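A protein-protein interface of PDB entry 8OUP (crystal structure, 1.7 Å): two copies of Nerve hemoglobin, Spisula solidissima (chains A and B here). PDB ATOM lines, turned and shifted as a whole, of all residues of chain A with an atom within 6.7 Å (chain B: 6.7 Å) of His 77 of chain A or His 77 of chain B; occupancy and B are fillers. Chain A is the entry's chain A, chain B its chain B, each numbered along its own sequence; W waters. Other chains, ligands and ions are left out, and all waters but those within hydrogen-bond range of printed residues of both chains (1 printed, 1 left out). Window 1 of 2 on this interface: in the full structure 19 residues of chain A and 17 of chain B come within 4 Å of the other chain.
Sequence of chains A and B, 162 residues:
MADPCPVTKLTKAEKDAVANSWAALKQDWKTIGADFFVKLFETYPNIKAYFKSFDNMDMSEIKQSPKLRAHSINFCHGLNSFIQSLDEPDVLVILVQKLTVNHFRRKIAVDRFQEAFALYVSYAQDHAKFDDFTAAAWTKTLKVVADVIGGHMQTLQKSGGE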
ATOM      1  N   TRP A  22      16.759   9.982  -9.895  1.00  0.00           N
ATOM      2  CA  TRP A  22      17.644  10.665  -8.966  1.00  0.00           C
ATOM      3  C   TRP A  22      18.556  11.662  -9.676  1.00  0.00           C
ATOM      4  O   TRP A  22      18.749  12.748  -9.159  1.00  0.00           O
ATOM      5  CB  TRP A  22      18.418   9.622  -8.186  1.00  0.00           C
ATOM      6  CG  TRP A  22      19.334  10.227  -7.181  1.00  0.00           C
ATOM      7  CD1 TRP A  22      20.693  10.128  -7.158  1.00  0.00           C
ATOM      8  CD2 TRP A  22      18.963  11.101  -6.120  1.00  0.00           C
ATOM      9  NE1 TRP A  22      21.183  10.863  -6.109  1.00  0.00           N
ATOM     10  CE2 TRP A  22      20.162  11.440  -5.428  1.00  0.00           C
ATOM     11  CE3 TRP A  22      17.780  11.631  -5.625  1.00  0.00           C
ATOM     12  CZ2 TRP A  22      20.178  12.316  -4.347  1.00  0.00           C
ATOM     13  CZ3 TRP A  22      17.792  12.469  -4.537  1.00  0.00           C
ATOM     14  CH2 TRP A  22      18.989  12.803  -3.885  1.00  0.00           C
ATOM     15  N   LYS A  26      18.261  15.168  -7.954  1.00  0.00           N
ATOM     16  CA  LYS A  26      19.442  15.571  -7.198  1.00  0.00           C
ATOM     17  C   LYS A  26      19.679  17.042  -7.434  1.00  0.00           C
ATOM     18  O   LYS A  26      20.061  17.804  -6.541  1.00  0.00           O
ATOM     19  CB  LYS A  26      20.744  15.081  -7.842  1.00  0.00           C
ATOM     20  CG  LYS A  26      21.341  13.792  -7.375  1.00  0.00           C
ATOM     21  CD  LYS A  26      22.371  13.337  -8.374  1.00  0.00           C
ATOM     22  CE  LYS A  26      23.777  13.763  -8.048  1.00  0.00           C
ATOM     23  NZ  LYS A  26      24.691  12.651  -8.371  1.00  0.00           N
ATOM     24  N   TRP A  29      17.437  19.431  -5.684  1.00  0.00           N
ATOM     25  CA  TRP A  29      17.371  19.296  -4.221  1.00  0.00           C
ATOM     26  C   TRP A  29      17.788  20.574  -3.495  1.00  0.00           C
ATOM     27  O   TRP A  29      17.288  20.856  -2.408  1.00  0.00           O
ATOM     28  CB  TRP A  29      18.213  18.099  -3.753  1.00  0.00           C
ATOM     29  CG  TRP A  29      17.806  17.603  -2.397  1.00  0.00           C
ATOM     30  CD1 TRP A  29      18.490  17.772  -1.221  1.00  0.00           C
ATOM     31  CD2 TRP A  29      16.559  16.988  -2.057  1.00  0.00           C
ATOM     32  NE1 TRP A  29      17.785  17.211  -0.195  1.00  0.00           N
ATOM     33  CE2 TRP A  29      16.603  16.719  -0.675  1.00  0.00           C
ATOM     34  CE3 TRP A  29      15.458  16.551  -2.816  1.00  0.00           C
ATOM     35  CZ2 TRP A  29      15.541  16.087  -0.030  1.00  0.00           C
ATOM     36  CZ3 TRP A  29      14.395  15.974  -2.169  1.00  0.00           C
ATOM     37  CH2 TRP A  29      14.444  15.750  -0.790  1.00  0.00           C
ATOM     38  N   SER A  72      19.926  18.642   4.927  1.00  0.00           N
ATOM     39  CA  SER A  72      19.359  18.346   3.622  1.00  0.00           C
ATOM     40  C   SER A  72      20.420  17.924   2.590  1.00  0.00           C
ATOM     41  O   SER A  72      20.216  16.976   1.829  1.00  0.00           O
ATOM     42  CB  SER A  72      18.544  19.534   3.202  1.00  0.00           C
ATOM     43  OG  SER A  72      17.974  19.290   1.936  1.00  0.00           O
ATOM     44  N   ILE A  73      21.594  18.564   2.615  1.00  0.00           N
ATOM     45  CA  ILE A  73      22.724  18.188   1.773  1.00  0.00           C
ATOM     46  C   ILE A  73      23.220  16.812   2.189  1.00  0.00           C
ATOM     47  O   ILE A  73      23.553  15.964   1.343  1.00  0.00           O
ATOM     48  CB  ILE A  73      23.830  19.262   1.871  1.00  0.00           C
ATOM     49  CG1 ILE A  73      23.565  20.399   0.889  1.00  0.00           C
ATOM     50  CG2 ILE A  73      25.224  18.666   1.674  1.00  0.00           C
ATOM     51  CD1 ILE A  73      22.134  20.866   0.872  1.00  0.00           C
ATOM     52  N   ASN A  74      23.327  16.597   3.498  1.00  0.00           N
ATOM     53  CA  ASN A  74      23.786  15.321   3.998  1.00  0.00           C
ATOM     54  C   ASN A  74      22.845  14.207   3.547  1.00  0.00           C
ATOM     55  O   ASN A  74      23.291  13.132   3.183  1.00  0.00           O
ATOM     56  CB  ASN A  74      23.939  15.321   5.501  1.00  0.00           C
ATOM     57  CG  ASN A  74      25.237  15.948   5.985  1.00  0.00           C
ATOM     58  OD1 ASN A  74      25.219  16.497   7.085  1.00  0.00           O
ATOM     59  ND2 ASN A  74      26.278  15.934   5.174  1.00  0.00           N
ATOM     60  N   PHE A  75      21.555  14.482   3.578  1.00  0.00           N
ATOM     61  CA  PHE A  75      20.538  13.537   3.138  1.00  0.00           C
ATOM     62  C   PHE A  75      20.712  13.186   1.666  1.00  0.00           C
ATOM     63  O   PHE A  75      20.743  12.013   1.261  1.00  0.00           O
ATOM     64  CB  PHE A  75      19.152  14.105   3.488  1.00  0.00           C
ATOM     65  CG  PHE A  75      17.979  13.311   2.965  1.00  0.00           C
ATOM     66  CD1 PHE A  75      17.475  13.563   1.701  1.00  0.00           C
ATOM     67  CD2 PHE A  75      17.362  12.329   3.731  1.00  0.00           C
ATOM     68  CE1 PHE A  75      16.390  12.861   1.194  1.00  0.00           C
ATOM     69  CE2 PHE A  75      16.240  11.667   3.239  1.00  0.00           C
ATOM     70  CZ  PHE A  75      15.807  11.877   1.944  1.00  0.00           C
ATOM     71  N   CYS A  76      20.818  14.168   0.782  1.00  0.00           N
ATOM     72  CA  CYS A  76      20.915  13.820  -0.624  1.00  0.00           C
ATOM     73  C   CYS A  76      22.281  13.191  -0.905  1.00  0.00           C
ATOM     74  O   CYS A  76      22.393  12.326  -1.754  1.00  0.00           O
ATOM     75  CB  CYS A  76      20.734  15.040  -1.497  1.00  0.00           C
ATOM     76  SG  CYS A  76      22.022  16.205  -1.063  1.00  0.00           S
ATOM     77  N   HIS A  77      23.351  13.607  -0.206  1.00  0.00           N
ATOM     78  CA  HIS A  77      24.617  12.929  -0.464  1.00  0.00           C
ATOM     79  C   HIS A  77      24.587  11.478  -0.005  1.00  0.00           C
ATOM     80  O   HIS A  77      25.179  10.592  -0.650  1.00  0.00           O
ATOM     81  CB  HIS A  77      25.772  13.731   0.141  1.00  0.00           C
ATOM     82  CG  HIS A  77      26.103  14.926  -0.696  1.00  0.00           C
ATOM     83  ND1 HIS A  77      27.276  15.141  -1.382  1.00  0.00           N
ATOM     84  CD2 HIS A  77      25.284  15.959  -1.005  1.00  0.00           C
ATOM     85  CE1 HIS A  77      27.181  16.294  -2.054  1.00  0.00           C
ATOM     86  NE2 HIS A  77      25.965  16.794  -1.854  1.00  0.00           N
ATOM     87  N   GLY A  78      24.001  11.239   1.162  1.00  0.00           N
ATOM     88  CA  GLY A  78      23.866   9.882   1.655  1.00  0.00           C
ATOM     89  C   GLY A  78      23.072   9.022   0.677  1.00  0.00           C
ATOM     90  O   GLY A  78      23.523   7.961   0.224  1.00  0.00           O
ATOM     91  N   LEU A  79      21.915   9.536   0.228  1.00  0.00           N
ATOM     92  CA  LEU A  79      21.121   8.808  -0.727  1.00  0.00           C
ATOM     93  C   LEU A  79      21.933   8.567  -2.006  1.00  0.00           C
ATOM     94  O   LEU A  79      21.942   7.472  -2.556  1.00  0.00           O
ATOM     95  CB  LEU A  79      19.850   9.640  -0.930  1.00  0.00           C
ATOM     96  CG  LEU A  79      18.784   8.980  -1.774  1.00  0.00           C
ATOM     97  CD1 LEU A  79      18.444   7.609  -1.222  1.00  0.00           C
ATOM     98  CD2 LEU A  79      17.552   9.870  -1.854  1.00  0.00           C
ATOM     99  N   ASN A  80      22.639   9.588  -2.494  1.00  0.00           N
ATOM    100  CA  ASN A  80      23.462   9.398  -3.677  1.00  0.00           C
ATOM    101  C   ASN A  80      24.467   8.266  -3.495  1.00  0.00           C
ATOM    102  O   ASN A  80      24.700   7.478  -4.423  1.00  0.00           O
ATOM    103  CB  ASN A  80      24.222  10.666  -4.043  1.00  0.00           C
ATOM    104  CG  ASN A  80      24.737  10.587  -5.466  1.00  0.00           C
ATOM    105  OD1 ASN A  80      23.971  10.787  -6.415  1.00  0.00           O
ATOM    106  ND2 ASN A  80      26.022  10.312  -5.611  1.00  0.00           N
ATOM    107  N   SER A  81      25.123   8.234  -2.326  1.00  0.00           N
ATOM    108  CA  SER A  81      26.136   7.228  -2.034  1.00  0.00           C
ATOM    109  C   SER A  81      25.535   5.829  -2.088  1.00  0.00           C
ATOM    110  O   SER A  81      26.193   4.897  -2.590  1.00  0.00           O
ATOM    111  CB  SER A  81      26.850   7.483  -0.696  1.00  0.00           C
ATOM    112  OG  SER A  81      26.082   7.149   0.448  1.00  0.00           O
ATOM    113  N   PHE A  82      24.285   5.700  -1.617  1.00  0.00           N
ATOM    114  CA  PHE A  82      23.597   4.411  -1.623  1.00  0.00           C
ATOM    115  C   PHE A  82      23.260   3.991  -3.047  1.00  0.00           C
ATOM    116  O   PHE A  82      23.540   2.851  -3.456  1.00  0.00           O
ATOM    117  CB  PHE A  82      22.358   4.435  -0.722  1.00  0.00           C
ATOM    118  CG  PHE A  82      22.604   4.884   0.701  1.00  0.00           C
ATOM    119  CD1 PHE A  82      23.840   4.765   1.309  1.00  0.00           C
ATOM    120  CD2 PHE A  82      21.575   5.435   1.446  1.00  0.00           C
ATOM    121  CE1 PHE A  82      24.053   5.267   2.580  1.00  0.00           C
ATOM    122  CE2 PHE A  82      21.778   5.926   2.714  1.00  0.00           C
ATOM    123  CZ  PHE A  82      23.016   5.822   3.291  1.00  0.00           C
ATOM    124  N   GLN A  84      24.576   4.981  -5.797  1.00  0.00           N
ATOM    125  CA  GLN A  84      25.812   4.713  -6.508  1.00  0.00           C
ATOM    126  C   GLN A  84      26.262   3.271  -6.276  1.00  0.00           C
ATOM    127  O   GLN A  84      26.911   2.682  -7.164  1.00  0.00           O
ATOM    128  CB  GLN A  84      26.895   5.687  -6.034  1.00  0.00           C
ATOM    129  CG  GLN A  84      28.239   5.465  -6.702  1.00  0.00           C
ATOM    130  CD  GLN A  84      29.243   6.542  -6.355  1.00  0.00           C
ATOM    131  OE1 GLN A  84      28.927   7.723  -6.338  1.00  0.00           O
ATOM    132  NE2 GLN A  84      30.478   6.147  -6.143  1.00  0.00           N
ATOM    133  N   TRP B  22      36.248  19.154 -10.710  1.00  0.00           N
ATOM    134  CA  TRP B  22      35.643  18.142  -9.857  1.00  0.00           C
ATOM    135  C   TRP B  22      34.498  17.445 -10.595  1.00  0.00           C
ATOM    136  O   TRP B  22      34.329  16.236 -10.514  1.00  0.00           O
ATOM    137  CB  TRP B  22      35.166  18.753  -8.554  1.00  0.00           C
ATOM    138  CG  TRP B  22      34.425  17.767  -7.707  1.00  0.00           C
ATOM    139  CD1 TRP B  22      33.115  17.782  -7.309  1.00  0.00           C
ATOM    140  CD2 TRP B  22      34.990  16.567  -7.178  1.00  0.00           C
ATOM    141  NE1 TRP B  22      32.846  16.699  -6.541  1.00  0.00           N
ATOM    142  CE2 TRP B  22      33.971  15.925  -6.446  1.00  0.00           C
ATOM    143  CE3 TRP B  22      36.274  16.023  -7.176  1.00  0.00           C
ATOM    144  CZ2 TRP B  22      34.209  14.733  -5.787  1.00  0.00           C
ATOM    145  CZ3 TRP B  22      36.512  14.862  -6.493  1.00  0.00           C
ATOM    146  CH2 TRP B  22      35.474  14.206  -5.841  1.00  0.00           C
ATOM    147  N   LYS B  26      34.911  13.429 -10.539  1.00  0.00           N
ATOM    148  CA  LYS B  26      34.028  12.672  -9.653  1.00  0.00           C
ATOM    149  C   LYS B  26      33.488  11.429 -10.364  1.00  0.00           C
ATOM    150  O   LYS B  26      33.345  10.370  -9.742  1.00  0.00           O
ATOM    151  CB  LYS B  26      32.899  13.548  -9.098  1.00  0.00           C
ATOM    152  CG  LYS B  26      31.861  13.918 -10.137  1.00  0.00           C
ATOM    153  CD  LYS B  26      30.470  14.094  -9.566  1.00  0.00           C
ATOM    154  CE  LYS B  26      30.270  15.397  -8.844  1.00  0.00           C
ATOM    155  NZ  LYS B  26      28.879  15.499  -8.355  1.00  0.00           N
ATOM    156  N   TRP B  29      36.284   8.958 -10.180  1.00  0.00           N
ATOM    157  CA  TRP B  29      36.673   8.628  -8.800  1.00  0.00           C
ATOM    158  C   TRP B  29      36.179   7.251  -8.413  1.00  0.00           C
ATOM    159  O   TRP B  29      36.757   6.542  -7.596  1.00  0.00           O
ATOM    160  CB  TRP B  29      36.153   9.684  -7.807  1.00  0.00           C
ATOM    161  CG  TRP B  29      36.918   9.593  -6.509  1.00  0.00           C
ATOM    162  CD1 TRP B  29      36.503   9.038  -5.349  1.00  0.00           C
ATOM    163  CD2 TRP B  29      38.239  10.090  -6.275  1.00  0.00           C
ATOM    164  NE1 TRP B  29      37.472   9.168  -4.395  1.00  0.00           N
ATOM    165  CE2 TRP B  29      38.573   9.765  -4.944  1.00  0.00           C
ATOM    166  CE3 TRP B  29      39.208  10.693  -7.068  1.00  0.00           C
ATOM    167  CZ2 TRP B  29      39.814  10.068  -4.411  1.00  0.00           C
ATOM    168  CZ3 TRP B  29      40.432  11.001  -6.539  1.00  0.00           C
ATOM    169  CH2 TRP B  29      40.733  10.696  -5.212  1.00  0.00           C
ATOM    170  N   SER B  72      36.428   5.730   0.191  1.00  0.00           N
ATOM    171  CA  SER B  72      36.696   6.520  -0.991  1.00  0.00           C
ATOM    172  C   SER B  72      35.429   7.228  -1.489  1.00  0.00           C
ATOM    173  O   SER B  72      35.487   8.376  -1.899  1.00  0.00           O
ATOM    174  CB  SER B  72      37.287   5.645  -2.010  1.00  0.00           C
ATOM    175  OG  SER B  72      37.480   6.331  -3.209  1.00  0.00           O
ATOM    176  N   ILE B  73      34.285   6.555  -1.353  1.00  0.00           N
ATOM    177  CA  ILE B  73      32.986   7.128  -1.688  1.00  0.00           C
ATOM    178  C   ILE B  73      32.645   8.235  -0.686  1.00  0.00           C
ATOM    179  O   ILE B  73      32.188   9.306  -1.122  1.00  0.00           O
ATOM    180  CB  ILE B  73      31.899   6.038  -1.713  1.00  0.00           C
ATOM    181  CG1 ILE B  73      32.132   5.057  -2.857  1.00  0.00           C
ATOM    182  CG2 ILE B  73      30.504   6.678  -1.743  1.00  0.00           C
ATOM    183  CD1 ILE B  73      31.298   3.790  -2.758  1.00  0.00           C
ATOM    184  N   ASN B  74      32.917   7.993   0.609  1.00  0.00           N
ATOM    185  CA  ASN B  74      32.685   8.956   1.700  1.00  0.00           C
ATOM    186  C   ASN B  74      33.545  10.203   1.401  1.00  0.00           C
ATOM    187  O   ASN B  74      33.081  11.346   1.567  1.00  0.00           O
ATOM    188  CB  ASN B  74      33.040   8.491   3.115  1.00  0.00           C
ATOM    189  CG  ASN B  74      32.181   7.409   3.763  1.00  0.00           C
ATOM    190  OD1 ASN B  74      32.683   6.511   4.481  1.00  0.00           O
ATOM    191  ND2 ASN B  74      30.896   7.561   3.573  1.00  0.00           N
ATOM    192  N   PHE B  75      34.796   9.986   0.968  1.00  0.00           N
ATOM    193  CA  PHE B  75      35.682  11.085   0.634  1.00  0.00           C
ATOM    194  C   PHE B  75      35.087  11.947  -0.474  1.00  0.00           C
ATOM    195  O   PHE B  75      35.049  13.181  -0.426  1.00  0.00           O
ATOM    196  CB  PHE B  75      37.068  10.531   0.287  1.00  0.00           C
ATOM    197  CG  PHE B  75      38.072  11.541  -0.177  1.00  0.00           C
ATOM    198  CD1 PHE B  75      38.885  12.208   0.729  1.00  0.00           C
ATOM    199  CD2 PHE B  75      38.246  11.760  -1.517  1.00  0.00           C
ATOM    200  CE1 PHE B  75      39.834  13.108   0.268  1.00  0.00           C
ATOM    201  CE2 PHE B  75      39.171  12.686  -1.981  1.00  0.00           C
ATOM    202  CZ  PHE B  75      39.967  13.343  -1.076  1.00  0.00           C
ATOM    203  N   CYS B  76      34.753  11.308  -1.576  1.00  0.00           N
ATOM    204  CA  CYS B  76      34.211  11.982  -2.727  1.00  0.00           C
ATOM    205  C   CYS B  76      32.945  12.763  -2.390  1.00  0.00           C
ATOM    206  O   CYS B  76      32.725  13.894  -2.830  1.00  0.00           O
ATOM    207  CB  CYS B  76      33.892  10.933  -3.759  1.00  0.00           C
ATOM    208  SG  CYS B  76      33.095  11.719  -5.148  1.00  0.00           S
ATOM    209  N   HIS B  77      32.067  12.114  -1.629  1.00  0.00           N
ATOM    210  CA  HIS B  77      30.825  12.773  -1.244  1.00  0.00           C
ATOM    211  C   HIS B  77      31.060  13.953  -0.311  1.00  0.00           C
ATOM    212  O   HIS B  77      30.401  15.004  -0.457  1.00  0.00           O
ATOM    213  CB  HIS B  77      29.793  11.803  -0.701  1.00  0.00           C
ATOM    214  CG  HIS B  77      29.227  10.931  -1.771  1.00  0.00           C
ATOM    215  ND1 HIS B  77      27.939  10.949  -2.227  1.00  0.00           N
ATOM    216  CD2 HIS B  77      29.887  10.057  -2.558  1.00  0.00           C
ATOM    217  CE1 HIS B  77      27.802  10.050  -3.199  1.00  0.00           C
ATOM    218  NE2 HIS B  77      28.988   9.502  -3.445  1.00  0.00           N
ATOM    219  N   GLY B  78      31.962  13.795   0.644  1.00  0.00           N
ATOM    220  CA  GLY B  78      32.331  14.886   1.511  1.00  0.00           C
ATOM    221  C   GLY B  78      32.847  16.048   0.680  1.00  0.00           C
ATOM    222  O   GLY B  78      32.423  17.187   0.860  1.00  0.00           O
ATOM    223  N   LEU B  79      33.837  15.789  -0.172  1.00  0.00           N
ATOM    224  CA  LEU B  79      34.406  16.850  -1.001  1.00  0.00           C
ATOM    225  C   LEU B  79      33.289  17.504  -1.819  1.00  0.00           C
ATOM    226  O   LEU B  79      33.199  18.737  -1.953  1.00  0.00           O
ATOM    227  CB  LEU B  79      35.463  16.324  -1.988  1.00  0.00           C
ATOM    228  CG  LEU B  79      36.859  16.065  -1.426  1.00  0.00           C
ATOM    229  CD1 LEU B  79      37.857  15.802  -2.540  1.00  0.00           C
ATOM    230  CD2 LEU B  79      37.313  17.212  -0.539  1.00  0.00           C
ATOM    231  N   ASN B  80      32.422  16.668  -2.397  1.00  0.00           N
ATOM    232  CA  ASN B  80      31.352  17.261  -3.200  1.00  0.00           C
ATOM    233  C   ASN B  80      30.488  18.205  -2.370  1.00  0.00           C
ATOM    234  O   ASN B  80      30.143  19.319  -2.852  1.00  0.00           O
ATOM    235  CB  ASN B  80      30.481  16.193  -3.817  1.00  0.00           C
ATOM    236  CG  ASN B  80      29.617  16.757  -4.918  1.00  0.00           C
ATOM    237  OD1 ASN B  80      30.084  16.920  -6.049  1.00  0.00           O
ATOM    238  ND2 ASN B  80      28.351  16.982  -4.598  1.00  0.00           N
ATOM    239  N   SER B  81      30.140  17.779  -1.162  1.00  0.00           N
ATOM    240  CA  SER B  81      29.275  18.591  -0.292  1.00  0.00           C
ATOM    241  C   SER B  81      29.932  19.949   0.017  1.00  0.00           C
ATOM    242  O   SER B  81      29.289  21.013   0.089  1.00  0.00           O
ATOM    243  CB  SER B  81      28.878  17.874   0.944  1.00  0.00           C
ATOM    244  OG  SER B  81      29.903  17.854   1.907  1.00  0.00           O
ATOM    245  N   PHE B  82      31.250  19.933   0.178  1.00  0.00           N
ATOM    246  CA  PHE B  82      31.967  21.173   0.445  1.00  0.00           C
ATOM    247  C   PHE B  82      31.996  22.067  -0.786  1.00  0.00           C
ATOM    248  O   PHE B  82      31.701  23.280  -0.678  1.00  0.00           O
ATOM    249  CB  PHE B  82      33.390  20.874   0.912  1.00  0.00           C
ATOM    250  CG  PHE B  82      33.490  19.955   2.100  1.00  0.00           C
ATOM    251  CD1 PHE B  82      32.453  19.725   2.987  1.00  0.00           C
ATOM    252  CD2 PHE B  82      34.691  19.315   2.311  1.00  0.00           C
ATOM    253  CE1 PHE B  82      32.570  18.820   4.029  1.00  0.00           C
ATOM    254  CE2 PHE B  82      34.821  18.398   3.349  1.00  0.00           C
ATOM    255  CZ  PHE B  82      33.774  18.173   4.220  1.00  0.00           C
ATOM    256  N   GLN B  84      30.033  22.101  -3.301  1.00  0.00           N
ATOM    257  CA  GLN B  84      28.694  22.599  -3.582  1.00  0.00           C
ATOM    258  C   GLN B  84      28.312  23.772  -2.682  1.00  0.00           C
ATOM    259  O   GLN B  84      27.381  24.525  -3.050  1.00  0.00           O
ATOM    260  CB  GLN B  84      27.705  21.465  -3.331  1.00  0.00           C
ATOM    261  CG  GLN B  84      26.275  21.754  -3.710  1.00  0.00           C
ATOM    262  CD  GLN B  84      25.509  20.476  -3.455  1.00  0.00           C
ATOM    263  OE1 GLN B  84      24.714  20.397  -2.521  1.00  0.00           O
ATOM    264  NE2 GLN B  84      25.815  19.463  -4.256  1.00  0.00           N
HETATM  265  O   HOH W   1      21.938  18.914  -2.223  1.00  0.00           O
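Among the printed residues, merely in contact across the chains: Ile 73 of chain A with Ser 81 of chain B, Ile 73 of chain A with Gln 84 of chain B, His 77 of chain A with Asn 80 of chain B, His 77 of chain A with Ser 81 of chain B, His 77 of chain A with Gln 84 of chain B, Asn 80 of chain A with His 77 of chain B, Ser 81 of chain A with Ile 73 of chain B, Ser 81 of chain A with His 77 of chain B and Gln 84 of chain A with Ile 73 of chain B.
Water W1 bridges the side-chain sulfur (SG) of Cys 76 of chain A (2.9 Å) and the side-chain amide oxygen (OE1) of Gln 84 of chain B (3.2 Å).
His 77 of chain B touches its own counterpart, His 77 of chain A.
His 77 of chain A touches Asn 80 of chain B, and with the chains exchanged Asn 80 of chain A touches His 77 of chain B.
His 77 of chain A touches Ser 81 of chain B, and with the chains exchanged Ser 81 of chain A touches His 77 of chain B.
His 77 of chain A touches Gln 84 of chain B, and with the chains exchanged Gln 84 of chain A touches His 77 of chain B.
15 positions are printed for both chains.
Of the 11 pairs that touch across the chains among the printed residues, 11 have their exchanged pair printed and touching as well.
Of the 15 printed residues of chain B, 5 touch a printed residue of chain A.
Hydrophobic or aromatic side chains of chain B within 4 Å of the printed part of chain A: Ile 73 and His 77.
Of the 15 printed residues of chain A, 5 touch a printed residue of chain B.
Among the printed residues, no Asp or Glu carboxylate lies within 4 Å of a Lys or Arg side-chain nitrogen of the other chain.
The backbone carbonyl oxygen (O) of His 77 of chain A lies within hydrogen-bond range of a ring nitrogen (ND1) of His 77 of chain B (3.2 Å).
The side-chain amide oxygen (OE1) of Gln 84 of chain A sits at hydrogen-bond distance from a ring nitrogen (NE2) of His 77 of chain B.
Cys 76 of chain A touches none of the printed residues of chain B.
His 77 of chain A touches just these residues of chain B: His 77 (3.2 Å), Asn 80 (2.9 Å), Ser 81 (3.4 Å) and Gln 84 (3.6 Å).
Of the printed residues of chain B, Asn 80 of chain A touches His 77 (3.0 Å).
Of the printed residues of chain B, Gln 84 of chain A touches Ile 73 and His 77.
Of the printed residues of chain A, Ile 73 of chain B touches Ser 81 (3.9 Å) and Gln 84 (3.8 Å).
Of the printed residues of chain A, His 77 of chain B touches His 77, Asn 80, Ser 81 and Gln 84.
Phe 82 of chain B touches none of the printed residues of chain A.
The nearest residue of chain B that does not touch His 77 of chain A is Gly 78 of chain B (5.3 Å).
The nearest residue of chain A that does not touch His 77 of chain B is Gly 78 of chain A (5.2 Å).
The nearest printed residue of chain B that does not touch Asn 80 of chain A is Ile 73 of chain B (6.4 Å).
The indole nitrogen of Trp 22 of chain B is in hydrogen-bond range of the side-chain amide oxygen of Asn 80 of chain B, 2.8 Å away.
NE1 of Trp 22 of chain A is in hydrogen-bond range of OD1 of Asn 80 of chain A, 2.8 Å away.
The side-chain amino group (NZ) of Lys 26 of chain A sits at hydrogen-bond distance from the side-chain amide oxygen (OD1) of Asn 80 of chain A, at 2.8 Å.
The backbone carbonyl oxygen (O) of Gly 78 of chain B lies within hydrogen-bond range of the side-chain hydroxyl (OG) of Ser 81 of chain B (2.8 Å).
The backbone carbonyl oxygen (O) of Gly 78 of chain A sits at hydrogen-bond distance from the side-chain hydroxyl (OG) of Ser 81 of chain A (2.7 Å).
OD1 of Asn 80 of chain B is in hydrogen-bond range of NZ of Lys 26 of chain B, 3.0 Å away.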
